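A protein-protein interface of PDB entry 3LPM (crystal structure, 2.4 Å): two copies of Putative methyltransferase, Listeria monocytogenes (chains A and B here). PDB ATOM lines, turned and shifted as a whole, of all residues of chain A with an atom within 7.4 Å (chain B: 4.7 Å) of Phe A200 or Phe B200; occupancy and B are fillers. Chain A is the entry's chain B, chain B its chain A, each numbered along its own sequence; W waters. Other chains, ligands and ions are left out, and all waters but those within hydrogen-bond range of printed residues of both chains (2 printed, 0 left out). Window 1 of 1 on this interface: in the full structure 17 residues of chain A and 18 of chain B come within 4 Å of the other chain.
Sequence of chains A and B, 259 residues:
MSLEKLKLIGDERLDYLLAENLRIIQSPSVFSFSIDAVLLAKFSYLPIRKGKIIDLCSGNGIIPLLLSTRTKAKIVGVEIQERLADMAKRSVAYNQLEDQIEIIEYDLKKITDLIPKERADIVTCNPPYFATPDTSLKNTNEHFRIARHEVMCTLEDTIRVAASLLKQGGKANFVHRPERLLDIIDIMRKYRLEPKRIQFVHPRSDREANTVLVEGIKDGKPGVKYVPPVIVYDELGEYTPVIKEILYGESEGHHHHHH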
ATOM      1  N   LEU A  39      16.778 -17.137  16.462  1.00  0.00           N
ATOM      2  CA  LEU A  39      16.502 -16.975  17.890  1.00  0.00           C
ATOM      3  C   LEU A  39      17.660 -17.395  18.752  1.00  0.00           C
ATOM      4  O   LEU A  39      17.918 -16.773  19.765  1.00  0.00           O
ATOM      5  CB  LEU A  39      15.242 -17.748  18.299  1.00  0.00           C
ATOM      6  CG  LEU A  39      13.937 -17.192  17.734  1.00  0.00           C
ATOM      7  CD1 LEU A  39      12.769 -18.062  18.139  1.00  0.00           C
ATOM      8  CD2 LEU A  39      13.709 -15.722  18.151  1.00  0.00           C
ATOM      9  N   PHE A  43      19.703 -14.993  21.290  1.00  0.00           N
ATOM     10  CA  PHE A  43      19.834 -15.454  22.669  1.00  0.00           C
ATOM     11  C   PHE A  43      21.278 -15.393  23.158  1.00  0.00           C
ATOM     12  O   PHE A  43      21.516 -15.064  24.314  1.00  0.00           O
ATOM     13  CB  PHE A  43      19.308 -16.898  22.747  1.00  0.00           C
ATOM     14  CG  PHE A  43      19.442 -17.579  24.111  1.00  0.00           C
ATOM     15  CD1 PHE A  43      18.579 -17.276  25.140  1.00  0.00           C
ATOM     16  CD2 PHE A  43      20.371 -18.587  24.302  1.00  0.00           C
ATOM     17  CE1 PHE A  43      18.660 -17.932  26.368  1.00  0.00           C
ATOM     18  CE2 PHE A  43      20.462 -19.283  25.543  1.00  0.00           C
ATOM     19  CZ  PHE A  43      19.595 -18.943  26.576  1.00  0.00           C
ATOM     20  N   PRO A 178      11.240 -28.680  24.349  1.00  0.00           N
ATOM     21  CA  PRO A 178      10.917 -28.543  25.773  1.00  0.00           C
ATOM     22  C   PRO A 178      10.668 -29.851  26.495  1.00  0.00           C
ATOM     23  O   PRO A 178      11.038 -29.983  27.652  1.00  0.00           O
ATOM     24  CB  PRO A 178       9.636 -27.720  25.750  1.00  0.00           C
ATOM     25  CG  PRO A 178       9.726 -26.948  24.542  1.00  0.00           C
ATOM     26  CD  PRO A 178      10.358 -27.833  23.534  1.00  0.00           C
ATOM     27  N   GLU A 179      10.055 -30.818  25.824  1.00  0.00           N
ATOM     28  CA  GLU A 179       9.815 -32.109  26.455  1.00  0.00           C
ATOM     29  C   GLU A 179      11.121 -32.783  26.910  1.00  0.00           C
ATOM     30  O   GLU A 179      11.105 -33.612  27.808  1.00  0.00           O
ATOM     31  CB  GLU A 179       8.939 -33.041  25.580  1.00  0.00           C
ATOM     32  CG  GLU A 179       9.487 -33.405  24.187  1.00  0.00           C
ATOM     33  CD  GLU A 179       9.002 -32.476  23.063  1.00  0.00           C
ATOM     34  OE1 GLU A 179       8.473 -31.368  23.349  1.00  0.00           O
ATOM     35  OE2 GLU A 179       9.156 -32.867  21.878  1.00  0.00           O
ATOM     36  N   LEU A 181      13.849 -31.008  28.046  1.00  0.00           N
ATOM     37  CA  LEU A 181      14.585 -30.054  28.903  1.00  0.00           C
ATOM     38  C   LEU A 181      15.187 -30.595  30.208  1.00  0.00           C
ATOM     39  O   LEU A 181      16.304 -30.232  30.566  1.00  0.00           O
ATOM     40  CB  LEU A 181      13.730 -28.810  29.188  1.00  0.00           C
ATOM     41  CG  LEU A 181      14.284 -27.733  30.123  1.00  0.00           C
ATOM     42  CD1 LEU A 181      15.557 -27.151  29.540  1.00  0.00           C
ATOM     43  CD2 LEU A 181      13.260 -26.644  30.389  1.00  0.00           C
ATOM     44  N   ILE A 198      17.291 -19.634  30.651  1.00  0.00           N
ATOM     45  CA  ILE A 198      16.380 -20.431  29.833  1.00  0.00           C
ATOM     46  C   ILE A 198      15.329 -19.527  29.207  1.00  0.00           C
ATOM     47  O   ILE A 198      14.785 -18.649  29.874  1.00  0.00           O
ATOM     48  CB  ILE A 198      15.728 -21.570  30.657  1.00  0.00           C
ATOM     49  CG1 ILE A 198      16.782 -22.645  31.000  1.00  0.00           C
ATOM     50  CG2 ILE A 198      14.543 -22.185  29.890  1.00  0.00           C
ATOM     51  CD1 ILE A 198      16.359 -23.674  32.021  1.00  0.00           C
ATOM     52  N   GLN A 199      15.078 -19.721  27.913  1.00  0.00           N
ATOM     53  CA  GLN A 199      14.055 -18.940  27.204  1.00  0.00           C
ATOM     54  C   GLN A 199      13.114 -19.846  26.433  1.00  0.00           C
ATOM     55  O   GLN A 199      13.559 -20.661  25.614  1.00  0.00           O
ATOM     56  CB  GLN A 199      14.699 -17.932  26.275  1.00  0.00           C
ATOM     57  CG  GLN A 199      13.707 -17.094  25.498  1.00  0.00           C
ATOM     58  CD  GLN A 199      14.385 -15.973  24.734  1.00  0.00           C
ATOM     59  OE1 GLN A 199      15.269 -16.210  23.912  1.00  0.00           O
ATOM     60  NE2 GLN A 199      13.977 -14.737  25.008  1.00  0.00           N
ATOM     61  N   PHE A 200      11.817 -19.721  26.710  1.00  0.00           N
ATOM     62  CA  PHE A 200      10.822 -20.555  26.049  1.00  0.00           C
ATOM     63  C   PHE A 200      10.317 -19.835  24.827  1.00  0.00           C
ATOM     64  O   PHE A 200      10.222 -18.600  24.830  1.00  0.00           O
ATOM     65  CB  PHE A 200       9.676 -20.925  27.009  1.00  0.00           C
ATOM     66  CG  PHE A 200      10.092 -21.897  28.074  1.00  0.00           C
ATOM     67  CD1 PHE A 200      10.066 -23.260  27.826  1.00  0.00           C
ATOM     68  CD2 PHE A 200      10.571 -21.446  29.288  1.00  0.00           C
ATOM     69  CE1 PHE A 200      10.494 -24.175  28.793  1.00  0.00           C
ATOM     70  CE2 PHE A 200      11.008 -22.352  30.264  1.00  0.00           C
ATOM     71  CZ  PHE A 200      10.969 -23.719  30.016  1.00  0.00           C
ATOM     72  N   VAL A 201      10.024 -20.602  23.779  1.00  0.00           N
ATOM     73  CA  VAL A 201       9.401 -20.054  22.578  1.00  0.00           C
ATOM     74  C   VAL A 201       7.985 -20.613  22.498  1.00  0.00           C
ATOM     75  O   VAL A 201       7.788 -21.813  22.667  1.00  0.00           O
ATOM     76  CB  VAL A 201      10.196 -20.426  21.291  1.00  0.00           C
ATOM     77  CG1 VAL A 201       9.654 -19.690  20.072  1.00  0.00           C
ATOM     78  CG2 VAL A 201      11.660 -20.116  21.455  1.00  0.00           C
ATOM     79  N   HIS A 202       7.003 -19.747  22.263  1.00  0.00           N
ATOM     80  CA  HIS A 202       5.608 -20.175  22.134  1.00  0.00           C
ATOM     81  C   HIS A 202       5.045 -19.631  20.811  1.00  0.00           C
ATOM     82  O   HIS A 202       5.054 -18.416  20.598  1.00  0.00           O
ATOM     83  CB  HIS A 202       4.751 -19.665  23.312  1.00  0.00           C
ATOM     84  CG  HIS A 202       5.193 -20.149  24.663  1.00  0.00           C
ATOM     85  ND1 HIS A 202       4.546 -21.163  25.345  1.00  0.00           N
ATOM     86  CD2 HIS A 202       6.193 -19.735  25.474  1.00  0.00           C
ATOM     87  CE1 HIS A 202       5.144 -21.369  26.505  1.00  0.00           C
ATOM     88  NE2 HIS A 202       6.155 -20.523  26.603  1.00  0.00           N
ATOM     89  N   GLU A 208       1.369 -23.901  24.208  1.00  0.00           N
ATOM     90  CA  GLU A 208       2.507 -24.302  24.997  1.00  0.00           C
ATOM     91  C   GLU A 208       3.814 -24.148  24.222  1.00  0.00           C
ATOM     92  O   GLU A 208       3.803 -23.888  23.019  1.00  0.00           O
ATOM     93  CB  GLU A 208       2.324 -25.732  25.497  1.00  0.00           C
ATOM     94  CG  GLU A 208       1.285 -26.552  24.752  1.00  0.00           C
ATOM     95  CD  GLU A 208       1.237 -27.989  25.238  1.00  0.00           C
ATOM     96  OE1 GLU A 208       0.209 -28.381  25.853  1.00  0.00           O
ATOM     97  OE2 GLU A 208       2.244 -28.710  25.017  1.00  0.00           O
ATOM     98  N   ALA A 209       4.940 -24.302  24.917  1.00  0.00           N
ATOM     99  CA  ALA A 209       6.256 -24.147  24.294  1.00  0.00           C
ATOM    100  C   ALA A 209       6.587 -25.334  23.383  1.00  0.00           C
ATOM    101  O   ALA A 209       6.352 -26.481  23.754  1.00  0.00           O
ATOM    102  CB  ALA A 209       7.331 -23.969  25.356  1.00  0.00           C
ATOM    103  N   ASN A 210       7.106 -25.055  22.185  1.00  0.00           N
ATOM    104  CA  ASN A 210       7.665 -26.108  21.321  1.00  0.00           C
ATOM    105  C   ASN A 210       9.190 -26.039  21.176  1.00  0.00           C
ATOM    106  O   ASN A 210       9.828 -27.011  20.764  1.00  0.00           O
ATOM    107  CB  ASN A 210       6.982 -26.150  19.947  1.00  0.00           C
ATOM    108  CG  ASN A 210       7.047 -24.820  19.203  1.00  0.00           C
ATOM    109  OD1 ASN A 210       7.732 -23.882  19.611  1.00  0.00           O
ATOM    110  ND2 ASN A 210       6.327 -24.742  18.096  1.00  0.00           N
ATOM    111  N   THR A 211       9.763 -24.894  21.538  1.00  0.00           N
ATOM    112  CA  THR A 211      11.204 -24.665  21.453  1.00  0.00           C
ATOM    113  C   THR A 211      11.625 -24.061  22.776  1.00  0.00           C
ATOM    114  O   THR A 211      10.901 -23.222  23.322  1.00  0.00           O
ATOM    115  CB  THR A 211      11.542 -23.674  20.295  1.00  0.00           C
ATOM    116  OG1 THR A 211      11.087 -24.208  19.050  1.00  0.00           O
ATOM    117  CG2 THR A 211      13.026 -23.400  20.179  1.00  0.00           C
ATOM    118  N   VAL A 212      12.765 -24.502  23.304  1.00  0.00           N
ATOM    119  CA  VAL A 212      13.377 -23.833  24.442  1.00  0.00           C
ATOM    120  C   VAL A 212      14.870 -23.584  24.200  1.00  0.00           C
ATOM    121  O   VAL A 212      15.574 -24.440  23.670  1.00  0.00           O
ATOM    122  CB  VAL A 212      13.112 -24.568  25.791  1.00  0.00           C
ATOM    123  CG1 VAL A 212      13.804 -25.914  25.855  1.00  0.00           C
ATOM    124  CG2 VAL A 212      13.546 -23.707  26.952  1.00  0.00           C
ATOM    125  N   LEU A 213      15.327 -22.390  24.567  1.00  0.00           N
ATOM    126  CA  LEU A 213      16.745 -22.013  24.480  1.00  0.00           C
ATOM    127  C   LEU A 213      17.416 -22.166  25.845  1.00  0.00           C
ATOM    128  O   LEU A 213      16.829 -21.834  26.874  1.00  0.00           O
ATOM    129  CB  LEU A 213      16.877 -20.572  23.967  1.00  0.00           C
ATOM    130  CG  LEU A 213      16.152 -20.303  22.647  1.00  0.00           C
ATOM    131  CD1 LEU A 213      16.289 -18.881  22.198  1.00  0.00           C
ATOM    132  CD2 LEU A 213      16.693 -21.199  21.577  1.00  0.00           C
ATOM    133  N   VAL A 224      19.217 -20.413  37.829  1.00  0.00           N
ATOM    134  CA  VAL A 224      18.661 -20.077  36.552  1.00  0.00           C
ATOM    135  C   VAL A 224      17.858 -18.816  36.571  1.00  0.00           C
ATOM    136  O   VAL A 224      17.195 -18.513  37.516  1.00  0.00           O
ATOM    137  CB  VAL A 224      17.750 -21.137  36.042  1.00  0.00           C
ATOM    138  CG1 VAL A 224      17.266 -20.764  34.697  1.00  0.00           C
ATOM    139  CG2 VAL A 224      18.423 -22.420  36.000  1.00  0.00           C
ATOM    140  N   LYS A 225      17.945 -18.079  35.492  1.00  0.00           N
ATOM    141  CA  LYS A 225      17.055 -16.963  35.207  1.00  0.00           C
ATOM    142  C   LYS A 225      16.238 -17.399  34.008  1.00  0.00           C
ATOM    143  O   LYS A 225      16.804 -17.809  33.002  1.00  0.00           O
ATOM    144  CB  LYS A 225      17.860 -15.713  34.854  1.00  0.00           C
ATOM    145  CG  LYS A 225      18.420 -14.947  36.048  1.00  0.00           C
ATOM    146  CD  LYS A 225      19.806 -14.361  35.726  1.00  0.00           C
ATOM    147  CE  LYS A 225      20.154 -13.151  36.610  1.00  0.00           C
ATOM    148  NZ  LYS A 225      19.878 -11.836  35.925  1.00  0.00           N
ATOM    149  N   TYR A 226      14.918 -17.340  34.120  1.00  0.00           N
ATOM    150  CA  TYR A 226      14.015 -17.674  33.015  1.00  0.00           C
ATOM    151  C   TYR A 226      13.706 -16.406  32.279  1.00  0.00           C
ATOM    152  O   TYR A 226      12.966 -15.538  32.756  1.00  0.00           O
ATOM    153  CB  TYR A 226      12.747 -18.401  33.502  1.00  0.00           C
ATOM    154  CG  TYR A 226      13.141 -19.684  34.161  1.00  0.00           C
ATOM    155  CD1 TYR A 226      13.230 -20.853  33.435  1.00  0.00           C
ATOM    156  CD2 TYR A 226      13.507 -19.705  35.496  1.00  0.00           C
ATOM    157  CE1 TYR A 226      13.633 -22.026  34.038  1.00  0.00           C
ATOM    158  CE2 TYR A 226      13.920 -20.841  36.087  1.00  0.00           C
ATOM    159  CZ  TYR A 226      13.992 -22.013  35.361  1.00  0.00           C
ATOM    160  OH  TYR A 226      14.406 -23.181  35.985  1.00  0.00           O
ATOM    161  N   VAL A 227      14.311 -16.303  31.110  1.00  0.00           N
ATOM    162  CA  VAL A 227      14.279 -15.088  30.312  1.00  0.00           C
ATOM    163  C   VAL A 227      12.868 -14.898  29.761  1.00  0.00           C
ATOM    164  O   VAL A 227      12.141 -15.881  29.651  1.00  0.00           O
ATOM    165  CB  VAL A 227      15.407 -15.174  29.226  1.00  0.00           C
ATOM    166  CG1 VAL A 227      15.047 -14.439  27.944  1.00  0.00           C
ATOM    167  CG2 VAL A 227      16.717 -14.656  29.814  1.00  0.00           C
ATOM    168  N   PRO A 228      12.457 -13.640  29.457  1.00  0.00           N
ATOM    169  CA  PRO A 228      11.126 -13.458  28.882  1.00  0.00           C
ATOM    170  C   PRO A 228      10.890 -14.363  27.672  1.00  0.00           C
ATOM    171  O   PRO A 228      11.770 -14.483  26.812  1.00  0.00           O
ATOM    172  CB  PRO A 228      11.093 -11.979  28.468  1.00  0.00           C
ATOM    173  CG  PRO A 228      12.442 -11.429  28.750  1.00  0.00           C
ATOM    174  CD  PRO A 228      13.105 -12.344  29.725  1.00  0.00           C
ATOM    175  N   PRO A 229       9.712 -15.014  27.614  1.00  0.00           N
ATOM    176  CA  PRO A 229       9.450 -15.936  26.523  1.00  0.00           C
ATOM    177  C   PRO A 229       9.337 -15.200  25.194  1.00  0.00           C
ATOM    178  O   PRO A 229       8.979 -14.019  25.160  1.00  0.00           O
ATOM    179  CB  PRO A 229       8.095 -16.532  26.892  1.00  0.00           C
ATOM    180  CG  PRO A 229       7.419 -15.449  27.694  1.00  0.00           C
ATOM    181  CD  PRO A 229       8.513 -14.778  28.451  1.00  0.00           C
ATOM    182  N   VAL A 230       9.649 -15.907  24.115  1.00  0.00           N
ATOM    183  CA  VAL A 230       9.357 -15.425  22.775  1.00  0.00           C
ATOM    184  C   VAL A 230       7.984 -15.943  22.337  1.00  0.00           C
ATOM    185  O   VAL A 230       7.692 -17.141  22.469  1.00  0.00           O
ATOM    186  CB  VAL A 230      10.422 -15.898  21.776  1.00  0.00           C
ATOM    187  CG1 VAL A 230      10.187 -15.262  20.415  1.00  0.00           C
ATOM    188  CG2 VAL A 230      11.789 -15.545  22.287  1.00  0.00           C
ATOM    189  N   ILE A 231       7.144 -15.034  21.842  1.00  0.00           N
ATOM    190  CA  ILE A 231       5.888 -15.418  21.202  1.00  0.00           C
ATOM    191  C   ILE A 231       6.084 -15.154  19.730  1.00  0.00           C
ATOM    192  O   ILE A 231       6.371 -14.030  19.359  1.00  0.00           O
ATOM    193  CB  ILE A 231       4.672 -14.579  21.686  1.00  0.00           C
ATOM    194  CG1 ILE A 231       4.634 -14.423  23.220  1.00  0.00           C
ATOM    195  CG2 ILE A 231       3.364 -15.152  21.120  1.00  0.00           C
ATOM    196  CD1 ILE A 231       4.603 -15.749  24.019  1.00  0.00           C
ATOM    197  N   LEU B 181      13.184 -23.580  41.170  1.00  0.00           N
ATOM    198  CA  LEU B 181      12.505 -24.591  40.358  1.00  0.00           C
ATOM    199  C   LEU B 181      13.263 -25.913  40.207  1.00  0.00           C
ATOM    200  O   LEU B 181      12.714 -26.969  40.495  1.00  0.00           O
ATOM    201  CB  LEU B 181      12.105 -24.025  38.996  1.00  0.00           C
ATOM    202  CG  LEU B 181      11.391 -24.909  37.969  1.00  0.00           C
ATOM    203  CD1 LEU B 181      10.221 -25.623  38.599  1.00  0.00           C
ATOM    204  CD2 LEU B 181      10.933 -24.088  36.742  1.00  0.00           C
ATOM    205  N   ILE B 198       4.007 -26.804  33.935  1.00  0.00           N
ATOM    206  CA  ILE B 198       4.780 -25.716  34.483  1.00  0.00           C
ATOM    207  C   ILE B 198       4.335 -24.451  33.792  1.00  0.00           C
ATOM    208  O   ILE B 198       4.190 -24.411  32.566  1.00  0.00           O
ATOM    209  CB  ILE B 198       6.270 -25.974  34.317  1.00  0.00           C
ATOM    210  CG1 ILE B 198       6.754 -26.923  35.427  1.00  0.00           C
ATOM    211  CG2 ILE B 198       7.027 -24.704  34.407  1.00  0.00           C
ATOM    212  CD1 ILE B 198       8.149 -27.442  35.220  1.00  0.00           C
ATOM    213  N   GLN B 199       4.051 -23.428  34.591  1.00  0.00           N
ATOM    214  CA  GLN B 199       3.634 -22.152  34.056  1.00  0.00           C
ATOM    215  C   GLN B 199       4.492 -21.074  34.669  1.00  0.00           C
ATOM    216  O   GLN B 199       4.646 -21.022  35.891  1.00  0.00           O
ATOM    217  CB  GLN B 199       2.172 -21.874  34.369  1.00  0.00           C
ATOM    218  CG  GLN B 199       1.660 -20.593  33.690  1.00  0.00           C
ATOM    219  CD  GLN B 199       0.154 -20.456  33.710  1.00  0.00           C
ATOM    220  OE1 GLN B 199      -0.468 -20.493  34.767  1.00  0.00           O
ATOM    221  NE2 GLN B 199      -0.442 -20.297  32.539  1.00  0.00           N
ATOM    222  N   PHE B 200       5.023 -20.200  33.818  1.00  0.00           N
ATOM    223  CA  PHE B 200       5.832 -19.090  34.269  1.00  0.00           C
ATOM    224  C   PHE B 200       4.989 -17.843  34.301  1.00  0.00           C
ATOM    225  O   PHE B 200       4.124 -17.633  33.438  1.00  0.00           O
ATOM    226  CB  PHE B 200       7.083 -18.905  33.387  1.00  0.00           C
ATOM    227  CG  PHE B 200       8.109 -19.991  33.581  1.00  0.00           C
ATOM    228  CD1 PHE B 200       8.999 -19.932  34.639  1.00  0.00           C
ATOM    229  CD2 PHE B 200       8.150 -21.093  32.729  1.00  0.00           C
ATOM    230  CE1 PHE B 200       9.934 -20.946  34.851  1.00  0.00           C
ATOM    231  CE2 PHE B 200       9.081 -22.115  32.934  1.00  0.00           C
ATOM    232  CZ  PHE B 200       9.976 -22.038  33.998  1.00  0.00           C
ATOM    233  N   VAL B 201       5.238 -17.034  35.324  1.00  0.00           N
ATOM    234  CA  VAL B 201       4.615 -15.736  35.456  1.00  0.00           C
ATOM    235  C   VAL B 201       5.689 -14.667  35.318  1.00  0.00           C
ATOM    236  O   VAL B 201       6.681 -14.668  36.052  1.00  0.00           O
ATOM    237  CB  VAL B 201       3.904 -15.560  36.814  1.00  0.00           C
ATOM    238  CG1 VAL B 201       3.007 -14.310  36.770  1.00  0.00           C
ATOM    239  CG2 VAL B 201       3.082 -16.782  37.138  1.00  0.00           C
ATOM    240  N   HIS B 202       5.468 -13.770  34.364  1.00  0.00           N
ATOM    241  CA  HIS B 202       6.338 -12.638  34.095  1.00  0.00           C
ATOM    242  C   HIS B 202       5.535 -11.363  34.332  1.00  0.00           C
ATOM    243  O   HIS B 202       4.414 -11.260  33.818  1.00  0.00           O
ATOM    244  CB  HIS B 202       6.803 -12.673  32.638  1.00  0.00           C
ATOM    245  CG  HIS B 202       7.578 -13.900  32.283  1.00  0.00           C
ATOM    246  ND1 HIS B 202       8.955 -13.928  32.260  1.00  0.00           N
ATOM    247  CD2 HIS B 202       7.171 -15.145  31.938  1.00  0.00           C
ATOM    248  CE1 HIS B 202       9.362 -15.130  31.902  1.00  0.00           C
ATOM    249  NE2 HIS B 202       8.299 -15.892  31.709  1.00  0.00           N
ATOM    250  N   ALA B 209      11.003 -14.026  34.693  1.00  0.00           N
ATOM    251  CA  ALA B 209       9.956 -14.588  35.544  1.00  0.00           C
ATOM    252  C   ALA B 209      10.269 -14.455  37.038  1.00  0.00           C
ATOM    253  O   ALA B 209      11.407 -14.673  37.473  1.00  0.00           O
ATOM    254  CB  ALA B 209       9.685 -16.041  35.176  1.00  0.00           C
ATOM    255  N   THR B 211       7.629 -15.674  39.331  1.00  0.00           N
ATOM    256  CA  THR B 211       6.812 -16.754  39.885  1.00  0.00           C
ATOM    257  C   THR B 211       6.700 -17.906  38.875  1.00  0.00           C
ATOM    258  O   THR B 211       6.560 -17.653  37.666  1.00  0.00           O
ATOM    259  CB  THR B 211       5.380 -16.233  40.237  1.00  0.00           C
ATOM    260  OG1 THR B 211       5.445 -15.318  41.334  1.00  0.00           O
ATOM    261  CG2 THR B 211       4.449 -17.362  40.619  1.00  0.00           C
ATOM    262  N   VAL B 212       6.750 -19.150  39.363  1.00  0.00           N
ATOM    263  CA  VAL B 212       6.392 -20.327  38.550  1.00  0.00           C
ATOM    264  C   VAL B 212       5.330 -21.239  39.223  1.00  0.00           C
ATOM    265  O   VAL B 212       5.399 -21.517  40.438  1.00  0.00           O
ATOM    266  CB  VAL B 212       7.645 -21.136  38.127  1.00  0.00           C
ATOM    267  CG1 VAL B 212       8.358 -21.808  39.348  1.00  0.00           C
ATOM    268  CG2 VAL B 212       7.295 -22.157  37.070  1.00  0.00           C
ATOM    269  N   TYR B 226       5.026 -27.139  28.987  1.00  0.00           N
ATOM    270  CA  TYR B 226       5.255 -25.787  29.466  1.00  0.00           C
ATOM    271  C   TYR B 226       4.135 -24.898  28.988  1.00  0.00           C
ATOM    272  O   TYR B 226       4.091 -24.441  27.845  1.00  0.00           O
ATOM    273  CB  TYR B 226       6.663 -25.267  29.129  1.00  0.00           C
ATOM    274  CG  TYR B 226       7.720 -26.118  29.795  1.00  0.00           C
ATOM    275  CD1 TYR B 226       8.232 -25.787  31.034  1.00  0.00           C
ATOM    276  CD2 TYR B 226       8.154 -27.291  29.197  1.00  0.00           C
ATOM    277  CE1 TYR B 226       9.183 -26.586  31.641  1.00  0.00           C
ATOM    278  CE2 TYR B 226       9.078 -28.081  29.793  1.00  0.00           C
ATOM    279  CZ  TYR B 226       9.599 -27.729  31.019  1.00  0.00           C
ATOM    280  OH  TYR B 226      10.544 -28.542  31.612  1.00  0.00           O
ATOM    281  N   PRO B 229       2.760 -18.918  29.389  1.00  0.00           N
ATOM    282  CA  PRO B 229       3.097 -18.092  30.519  1.00  0.00           C
ATOM    283  C   PRO B 229       2.130 -16.975  30.683  1.00  0.00           C
ATOM    284  O   PRO B 229       1.420 -16.612  29.782  1.00  0.00           O
ATOM    285  CB  PRO B 229       4.420 -17.526  30.106  1.00  0.00           C
ATOM    286  CG  PRO B 229       4.294 -17.372  28.725  1.00  0.00           C
ATOM    287  CD  PRO B 229       3.450 -18.455  28.195  1.00  0.00           C
ATOM    288  N   VAL B 230       2.116 -16.438  31.874  1.00  0.00           N
ATOM    289  CA  VAL B 230       1.238 -15.373  32.198  1.00  0.00           C
ATOM    290  C   VAL B 230       2.008 -14.099  32.271  1.00  0.00           C
ATOM    291  O   VAL B 230       3.000 -14.003  32.947  1.00  0.00           O
ATOM    292  CB  VAL B 230       0.638 -15.586  33.563  1.00  0.00           C
ATOM    293  CG1 VAL B 230      -0.268 -14.480  33.914  1.00  0.00           C
ATOM    294  CG2 VAL B 230      -0.079 -16.852  33.599  1.00  0.00           C
HETATM  295  O   HOH W   1      13.504 -15.744  36.540  1.00  0.00           O
HETATM  296  O   HOH W   2       5.734 -27.530  26.334  1.00  0.00           O
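O of Tyr B226 is in hydrogen-bond range of N of Ala A209. The backbone carbonyl oxygen (O) of Tyr A226 lies within hydrogen-bond range of the backbone NH (N) of Ala B209, at 3.1 Å.
O of Phe B200 lies within hydrogen-bond range of N of Val B230, 2.8 Å away. O of Val A230 sits at hydrogen-bond distance from N of His A202 (2.7 Å). O of Phe A200 is in hydrogen-bond range of N of Val A230 (2.8 Å). A ring nitrogen (ND1) of His B202 is in hydrogen-bond range of the backbone NH (N) of Ala B209 (3.2 Å). N of His B202 lies within hydrogen-bond range of O of Val B230 (2.9 Å). The side-chain amide nitrogen (NE2) of Gln A199 lies within hydrogen-bond range of the backbone carbonyl oxygen (O) of Pro A228.
Among the printed residues, pairs that only touch across the chains: Pro A178 with Tyr B226, Leu A181 with Tyr B226, Phe A200 with Phe B200, Phe A200 with Tyr B226, His A202 with Tyr B226, His A202 with Pro B229, Glu A208 with Tyr B226, Tyr A226 with Leu B181, Tyr A226 with Phe B200, Tyr A226 with His B202, Val A227 with His B202, Pro A228 with His B202, Pro A229 with His B202 and Pro A229 with Pro B229.
Of the printed residues of chain B, Val A227 touches His B202. Phe B200 touches just these residues of chain A: Phe A200 (3.3 Å) and Tyr A226 (3.5 Å). Of the printed residues of chain A, Ala B209 touches Tyr A226. Of the printed residues of chain A, Tyr B226 touches Pro A178, Leu A181, Phe A200, His A202, Glu A208 and Ala A209. Printed residues of chain A within 4 Å of Pro B229: His A202 (3.8 Å) and Pro A229 (3.8 Å). The nearest printed residue of chain B that does not touch Phe A200 is Ile B198 (6.0 Å). The nearest residue of chain A that does not touch Phe B200 is Ile A198 (6.1 Å). The nearest printed residue of chain B that does not touch Glu A208 is Pro B229 (6.7 Å).
Of the 12 printed residues of chain B, 6 touch a printed residue of chain A. Hydrophobic or aromatic side chains of chain B that line the printed part of chain A: Leu B181, Phe B200, His B202, Tyr B226 and Pro B229. Of the 24 printed residues of chain A, 10 touch a printed residue of chain B. Hydrophobic or aromatic side chains of chain A that line the printed part of chain B: Pro A178, Leu A181, Phe A200, His A202, Tyr A226 and Pro A229.
Leu A181 touches Tyr B226, and with the chains exchanged Tyr A226 touches Leu B181. His A202 touches Tyr B226, and with the chains exchanged Tyr A226 touches His B202. His A202 touches Pro B229, and with the chains exchanged Pro A229 touches His B202. Pro B229 touches its own counterpart, Pro A229. 12 positions are printed for both chains. Of the 16 pairs that touch across the chains among the printed residues, 12 have their exchanged pair printed and touching as well.
Water W1 bridges the backbone carbonyl oxygen (O) of Ala B209 (2.5 Å) and the backbone NH (N) of Tyr A226 (3.2 Å). Water W2 bridges N of Tyr B226 (2.8 Å) and O of Ala A209 (2.9 Å).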
